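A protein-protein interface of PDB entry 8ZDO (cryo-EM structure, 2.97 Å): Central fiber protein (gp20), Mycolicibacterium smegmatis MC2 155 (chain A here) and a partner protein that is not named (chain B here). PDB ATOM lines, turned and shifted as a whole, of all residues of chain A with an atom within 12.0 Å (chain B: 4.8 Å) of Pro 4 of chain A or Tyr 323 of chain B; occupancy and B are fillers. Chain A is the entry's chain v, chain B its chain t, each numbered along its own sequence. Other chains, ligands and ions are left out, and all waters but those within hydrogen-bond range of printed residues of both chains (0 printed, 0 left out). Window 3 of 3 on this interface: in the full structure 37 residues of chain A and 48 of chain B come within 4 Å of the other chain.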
ATOM      1  N   MET A   1      17.205 -24.214  27.652  1.00  0.00           N
ATOM      2  CA  MET A   1      17.428 -22.774  27.689  1.00  0.00           C
ATOM      3  C   MET A   1      16.827 -22.104  26.462  1.00  0.00           C
ATOM      4  O   MET A   1      17.103 -20.941  26.176  1.00  0.00           O
ATOM      5  CB  MET A   1      18.922 -22.464  27.786  1.00  0.00           C
ATOM      6  CG  MET A   1      19.243 -21.160  28.499  1.00  0.00           C
ATOM      7  SD  MET A   1      18.906 -21.228  30.269  1.00  0.00           S
ATOM      8  CE  MET A   1      18.565 -19.504  30.608  1.00  0.00           C
ATOM      9  N   THR A   2      16.000 -22.846  25.738  1.00  0.00           N
ATOM     10  CA  THR A   2      15.322 -22.332  24.561  1.00  0.00           C
ATOM     11  C   THR A   2      13.899 -21.927  24.910  1.00  0.00           C
ATOM     12  O   THR A   2      13.245 -22.546  25.751  1.00  0.00           O
ATOM     13  CB  THR A   2      15.300 -23.370  23.440  1.00  0.00           C
ATOM     14  OG1 THR A   2      14.543 -24.510  23.860  1.00  0.00           O
ATOM     15  CG2 THR A   2      16.711 -23.802  23.096  1.00  0.00           C
ATOM     16  N   MET A   3      13.426 -20.870  24.258  1.00  0.00           N
ATOM     17  CA  MET A   3      12.058 -20.421  24.438  1.00  0.00           C
ATOM     18  C   MET A   3      11.250 -20.831  23.218  1.00  0.00           C
ATOM     19  O   MET A   3      11.470 -20.278  22.131  1.00  0.00           O
ATOM     20  CB  MET A   3      12.012 -18.909  24.633  1.00  0.00           C
ATOM     21  CG  MET A   3      12.984 -18.413  25.692  1.00  0.00           C
ATOM     22  SD  MET A   3      12.953 -16.629  25.933  1.00  0.00           S
ATOM     23  CE  MET A   3      13.872 -16.076  24.503  1.00  0.00           C
ATOM     24  N   PRO A   4      10.343 -21.806  23.332  1.00  0.00           N
ATOM     25  CA  PRO A   4       9.586 -22.241  22.146  1.00  0.00           C
ATOM     26  C   PRO A   4       8.761 -21.138  21.513  1.00  0.00           C
ATOM     27  O   PRO A   4       8.608 -21.114  20.286  1.00  0.00           O
ATOM     28  CB  PRO A   4       8.708 -23.370  22.698  1.00  0.00           C
ATOM     29  CG  PRO A   4       9.461 -23.877  23.871  1.00  0.00           C
ATOM     30  CD  PRO A   4      10.090 -22.671  24.493  1.00  0.00           C
ATOM     31  N   ASN A   5       8.219 -20.226  22.311  1.00  0.00           N
ATOM     32  CA  ASN A   5       7.558 -19.055  21.761  1.00  0.00           C
ATOM     33  C   ASN A   5       8.607 -18.018  21.361  1.00  0.00           C
ATOM     34  O   ASN A   5       9.812 -18.208  21.539  1.00  0.00           O
ATOM     35  CB  ASN A   5       6.548 -18.497  22.759  1.00  0.00           C
ATOM     36  CG  ASN A   5       7.090 -18.441  24.168  1.00  0.00           C
ATOM     37  OD1 ASN A   5       8.253 -18.758  24.410  1.00  0.00           O
ATOM     38  ND2 ASN A   5       6.247 -18.039  25.110  1.00  0.00           N
ATOM     39  N   GLY A   6       8.149 -16.899  20.815  1.00  0.00           N
ATOM     40  CA  GLY A   6       9.070 -15.919  20.277  1.00  0.00           C
ATOM     41  C   GLY A   6       9.662 -15.012  21.333  1.00  0.00           C
ATOM     42  O   GLY A   6      10.166 -15.481  22.356  1.00  0.00           O
ATOM     43  N   SER A   7       9.614 -13.703  21.086  1.00  0.00           N
ATOM     44  CA  SER A   7      10.082 -12.734  22.064  1.00  0.00           C
ATOM     45  C   SER A   7       9.208 -12.692  23.309  1.00  0.00           C
ATOM     46  O   SER A   7       9.600 -12.067  24.299  1.00  0.00           O
ATOM     47  CB  SER A   7      10.149 -11.345  21.431  1.00  0.00           C
ATOM     48  OG  SER A   7       8.966 -11.061  20.707  1.00  0.00           O
ATOM     49  N   GLY A   8       8.039 -13.332  23.282  1.00  0.00           N
ATOM     50  CA  GLY A   8       7.169 -13.383  24.441  1.00  0.00           C
ATOM     51  C   GLY A   8       7.682 -14.246  25.571  1.00  0.00           C
ATOM     52  O   GLY A   8       7.092 -14.226  26.656  1.00  0.00           O
ATOM     53  N   GLY A   9       8.754 -15.007  25.344  1.00  0.00           N
ATOM     54  CA  GLY A   9       9.363 -15.770  26.417  1.00  0.00           C
ATOM     55  C   GLY A   9      10.129 -14.924  27.410  1.00  0.00           C
ATOM     56  O   GLY A   9      10.359 -15.369  28.540  1.00  0.00           O
ATOM     57  N   LEU A  10      10.530 -13.719  27.017  1.00  0.00           N
ATOM     58  CA  LEU A  10      11.219 -12.812  27.917  1.00  0.00           C
ATOM     59  C   LEU A  10      10.234 -12.173  28.890  1.00  0.00           C
ATOM     60  O   LEU A  10       9.027 -12.113  28.645  1.00  0.00           O
ATOM     61  CB  LEU A  10      11.951 -11.724  27.132  1.00  0.00           C
ATOM     62  CG  LEU A  10      13.047 -12.172  26.166  1.00  0.00           C
ATOM     63  CD1 LEU A  10      13.476 -11.011  25.290  1.00  0.00           C
ATOM     64  CD2 LEU A  10      14.234 -12.742  26.920  1.00  0.00           C
ATOM     65  N   ASP A  11      10.770 -11.688  30.008  1.00  0.00           N
ATOM     66  CA  ASP A  11       9.960 -11.026  31.017  1.00  0.00           C
ATOM     67  C   ASP A  11      10.166  -9.523  30.917  1.00  0.00           C
ATOM     68  O   ASP A  11      11.262  -9.039  31.230  1.00  0.00           O
ATOM     69  CB  ASP A  11      10.325 -11.523  32.413  1.00  0.00           C
ATOM     70  CG  ASP A  11      10.301 -13.034  32.515  1.00  0.00           C
ATOM     71  OD1 ASP A  11      11.245 -13.679  32.016  1.00  0.00           O
ATOM     72  OD2 ASP A  11       9.334 -13.578  33.090  1.00  0.00           O
ATOM     73  N   SER B 236      13.053 -22.371  14.680  1.00  0.00           N
ATOM     74  CA  SER B 236      11.680 -22.245  15.157  1.00  0.00           C
ATOM     75  C   SER B 236      11.629 -21.672  16.565  1.00  0.00           C
ATOM     76  O   SER B 236      10.806 -20.798  16.859  1.00  0.00           O
ATOM     77  CB  SER B 236      10.984 -23.605  15.103  1.00  0.00           C
ATOM     78  OG  SER B 236      11.842 -24.628  15.577  1.00  0.00           O
ATOM     79  N   VAL B 237      12.504 -22.140  17.445  1.00  0.00           N
ATOM     80  CA  VAL B 237      12.510 -21.716  18.837  1.00  0.00           C
ATOM     81  C   VAL B 237      13.516 -20.591  19.016  1.00  0.00           C
ATOM     82  O   VAL B 237      14.473 -20.450  18.250  1.00  0.00           O
ATOM     83  CB  VAL B 237      12.822 -22.894  19.783  1.00  0.00           C
ATOM     84  CG1 VAL B 237      11.811 -24.007  19.589  1.00  0.00           C
ATOM     85  CG2 VAL B 237      14.232 -23.405  19.550  1.00  0.00           C
ATOM     86  N   THR B 301      12.810 -29.744  16.373  1.00  0.00           N
ATOM     87  CA  THR B 301      11.930 -28.610  16.609  1.00  0.00           C
ATOM     88  C   THR B 301      11.279 -28.084  15.335  1.00  0.00           C
ATOM     89  O   THR B 301      10.562 -27.082  15.393  1.00  0.00           O
ATOM     90  CB  THR B 301      12.702 -27.475  17.289  1.00  0.00           C
ATOM     91  OG1 THR B 301      13.916 -27.224  16.572  1.00  0.00           O
ATOM     92  CG2 THR B 301      13.036 -27.845  18.724  1.00  0.00           C
ATOM     93  N   LEU B 321       6.627 -32.116  17.593  1.00  0.00           N
ATOM     94  CA  LEU B 321       6.561 -31.631  18.964  1.00  0.00           C
ATOM     95  C   LEU B 321       5.332 -30.756  19.168  1.00  0.00           C
ATOM     96  O   LEU B 321       5.071 -29.837  18.386  1.00  0.00           O
ATOM     97  CB  LEU B 321       7.823 -30.844  19.308  1.00  0.00           C
ATOM     98  CG  LEU B 321       9.089 -31.637  19.626  1.00  0.00           C
ATOM     99  CD1 LEU B 321      10.268 -30.696  19.766  1.00  0.00           C
ATOM    100  CD2 LEU B 321       8.905 -32.447  20.893  1.00  0.00           C
ATOM    101  N   LEU B 322       4.582 -31.042  20.227  1.00  0.00           N
ATOM    102  CA  LEU B 322       3.435 -30.249  20.642  1.00  0.00           C
ATOM    103  C   LEU B 322       3.702 -29.710  22.038  1.00  0.00           C
ATOM    104  O   LEU B 322       4.002 -30.481  22.956  1.00  0.00           O
ATOM    105  CB  LEU B 322       2.154 -31.085  20.623  1.00  0.00           C
ATOM    106  CG  LEU B 322       0.877 -30.408  21.118  1.00  0.00           C
ATOM    107  CD1 LEU B 322       0.526 -29.219  20.242  1.00  0.00           C
ATOM    108  CD2 LEU B 322      -0.267 -31.406  21.161  1.00  0.00           C
ATOM    109  N   TYR B 323       3.597 -28.396  22.199  1.00  0.00           N
ATOM    110  CA  TYR B 323       3.951 -27.731  23.445  1.00  0.00           C
ATOM    111  C   TYR B 323       2.704 -27.490  24.282  1.00  0.00           C
ATOM    112  O   TYR B 323       1.692 -27.000  23.773  1.00  0.00           O
ATOM    113  CB  TYR B 323       4.666 -26.410  23.170  1.00  0.00           C
ATOM    114  CG  TYR B 323       6.014 -26.584  22.519  1.00  0.00           C
ATOM    115  CD1 TYR B 323       7.136 -26.882  23.274  1.00  0.00           C
ATOM    116  CD2 TYR B 323       6.163 -26.459  21.146  1.00  0.00           C
ATOM    117  CE1 TYR B 323       8.368 -27.048  22.683  1.00  0.00           C
ATOM    118  CE2 TYR B 323       7.390 -26.621  20.546  1.00  0.00           C
ATOM    119  CZ  TYR B 323       8.491 -26.915  21.319  1.00  0.00           C
ATOM    120  OH  TYR B 323       9.719 -27.078  20.724  1.00  0.00           O
ATOM    121  N   GLY B 324       2.787 -27.829  25.565  1.00  0.00           N
ATOM    122  CA  GLY B 324       1.693 -27.623  26.486  1.00  0.00           C
ATOM    123  C   GLY B 324       1.630 -26.193  26.987  1.00  0.00           C
ATOM    124  O   GLY B 324       2.231 -25.273  26.432  1.00  0.00           O
ATOM    125  N   GLY B 325       0.869 -26.012  28.063  1.00  0.00           N
ATOM    126  CA  GLY B 325       0.719 -24.704  28.669  1.00  0.00           C
ATOM    127  C   GLY B 325       2.025 -24.124  29.173  1.00  0.00           C
ATOM    128  O   GLY B 325       2.737 -24.759  29.958  1.00  0.00           O
ATOM    129  N   PHE B 327       4.658 -23.625  27.396  1.00  0.00           N
ATOM    130  CA  PHE B 327       5.720 -24.101  26.514  1.00  0.00           C
ATOM    131  C   PHE B 327       6.874 -24.752  27.266  1.00  0.00           C
ATOM    132  O   PHE B 327       7.912 -25.040  26.661  1.00  0.00           O
ATOM    133  CB  PHE B 327       6.247 -22.976  25.615  1.00  0.00           C
ATOM    134  CG  PHE B 327       5.201 -22.383  24.717  1.00  0.00           C
ATOM    135  CD1 PHE B 327       4.385 -21.360  25.165  1.00  0.00           C
ATOM    136  CD2 PHE B 327       5.032 -22.850  23.428  1.00  0.00           C
ATOM    137  CE1 PHE B 327       3.422 -20.816  24.346  1.00  0.00           C
ATOM    138  CE2 PHE B 327       4.071 -22.308  22.603  1.00  0.00           C
ATOM    139  CZ  PHE B 327       3.265 -21.290  23.063  1.00  0.00           C
ATOM    140  N   GLU B 329       6.643 -27.759  28.666  1.00  0.00           N
ATOM    141  CA  GLU B 329       6.520 -29.177  28.368  1.00  0.00           C
ATOM    142  C   GLU B 329       6.286 -29.377  26.880  1.00  0.00           C
ATOM    143  O   GLU B 329       5.483 -28.665  26.267  1.00  0.00           O
ATOM    144  CB  GLU B 329       5.360 -29.800  29.146  1.00  0.00           C
ATOM    145  CG  GLU B 329       5.455 -29.666  30.648  1.00  0.00           C
ATOM    146  CD  GLU B 329       4.214 -30.185  31.341  1.00  0.00           C
ATOM    147  OE1 GLU B 329       3.269 -30.592  30.635  1.00  0.00           O
ATOM    148  OE2 GLU B 329       4.173 -30.169  32.586  1.00  0.00           O
ATOM    149  N   ASP B 330       6.978 -30.354  26.302  1.00  0.00           N
ATOM    150  CA  ASP B 330       6.780 -30.736  24.911  1.00  0.00           C
ATOM    151  C   ASP B 330       6.568 -32.238  24.829  1.00  0.00           C
ATOM    152  O   ASP B 330       7.344 -33.010  25.401  1.00  0.00           O
ATOM    153  CB  ASP B 330       7.968 -30.319  24.042  1.00  0.00           C
ATOM    154  CG  ASP B 330       9.299 -30.702  24.652  1.00  0.00           C
ATOM    155  OD1 ASP B 330       9.325 -31.065  25.846  1.00  0.00           O
ATOM    156  OD2 ASP B 330      10.322 -30.642  23.939  1.00  0.00           O
ATOM    157  N   LEU B 475      11.024 -18.908  31.341  1.00  0.00           N
ATOM    158  CA  LEU B 475      10.764 -20.124  30.574  1.00  0.00           C
ATOM    159  C   LEU B 475      12.057 -20.852  30.234  1.00  0.00           C
ATOM    160  O   LEU B 475      12.137 -22.084  30.348  1.00  0.00           O
ATOM    161  CB  LEU B 475       9.987 -19.779  29.305  1.00  0.00           C
ATOM    162  CG  LEU B 475       9.798 -20.873  28.254  1.00  0.00           C
ATOM    163  CD1 LEU B 475       9.199 -22.118  28.872  1.00  0.00           C
ATOM    164  CD2 LEU B 475       8.919 -20.364  27.133  1.00  0.00           C
ATOM    165  N   ARG B 479      13.103 -24.681  31.361  1.00  0.00           N
ATOM    166  CA  ARG B 479      13.453 -25.713  30.388  1.00  0.00           C
ATOM    167  C   ARG B 479      14.873 -26.228  30.607  1.00  0.00           C
ATOM    168  O   ARG B 479      15.126 -27.435  30.511  1.00  0.00           O
ATOM    169  CB  ARG B 479      13.271 -25.176  28.970  1.00  0.00           C
ATOM    170  CG  ARG B 479      11.815 -24.946  28.597  1.00  0.00           C
ATOM    171  CD  ARG B 479      11.629 -24.829  27.097  1.00  0.00           C
ATOM    172  NE  ARG B 479      12.010 -26.050  26.401  1.00  0.00           N
ATOM    173  CZ  ARG B 479      11.163 -26.839  25.757  1.00  0.00           C
ATOM    174  NH1 ARG B 479       9.872 -26.563  25.697  1.00  0.00           N
ATOM    175  NH2 ARG B 479      11.622 -27.932  25.157  1.00  0.00           N
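NH1 of Arg 479 of chain B lies within hydrogen-bond range of O of Phe 327 of chain B, at 2.7 Å. The side-chain carboxylate of Asp 330 of chain B is in salt-bridge range of the guanidinium group of Arg 479 of chain B, at 3.2 Å.
Among the printed residues, pairs that only touch across the chains: Thr 2 of chain A with Arg 479 of chain B (3.1 Å), Asn 5 of chain A with Leu 475 of chain B (3.2 Å), Pro 4 of chain A with Arg 479 of chain B (3.3 Å), Pro 4 of chain A with Phe 327 of chain B (3.4 Å), Pro 4 of chain A with Tyr 323 of chain B (3.6 Å), Pro 4 of chain A with Leu 475 of chain B (3.7 Å), Met 3 of chain A with Val 237 of chain B (3.7 Å), Asn 5 of chain A with Phe 327 of chain B (3.8 Å) and Pro 4 of chain A with Val 237 of chain B (3.8 Å).
Printed residues of chain B within 4 Å of Thr 2 of chain A: Arg 479 (3.1 Å). Printed residues of chain B within 4 Å of Met 3 of chain A: Val 237 (3.7 Å). Pro 4 of chain A touches five residues of chain B. Of the printed residues of chain B, Asn 5 of chain A touches Phe 327 and Leu 475. Gly 6 of chain A touches none of the printed residues of chain B. Gly 9 of chain A touches none of the printed residues of chain B. No residue of chain A comes within 4 Å of Ser 236 of chain B. Val 237 of chain B touches just these residues of chain A: Met 3 (3.7 Å) and Pro 4 (3.8 Å). No residue of chain A comes within 4 Å of Leu 321 of chain B. No residue of chain A comes within 4 Å of Leu 322 of chain B. Tyr 323 of chain B touches just one residue of chain A: Pro 4. No residue of chain A comes within 4 Å of Gly 324 of chain B. No residue of chain A comes within 4 Å of Gly 325 of chain B. Printed residues of chain A within 4 Å of Arg 479 of chain B: Thr 2 (3.1 Å) and Pro 4 (3.3 Å). The nearest residue of chain B that does not touch Pro 4 of chain A is Ser 236 of chain B (4.1 Å). The nearest residue of chain A that does not touch Tyr 323 of chain B is Thr 2 of chain A (6.3 Å).
Hydrophobic or aromatic side chains of chain B within 4 Å of the printed part of chain A: Val 237, Tyr 323, Phe 327 and Leu 475. Of the 11 printed residues of chain A, 4 touch a printed residue of chain B. Among the printed residues, 9 pairs touch across the chains. Among the printed residues, no Asp or Glu carboxylate lies within 4 Å of a Lys or Arg side-chain nitrogen of the other chain.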
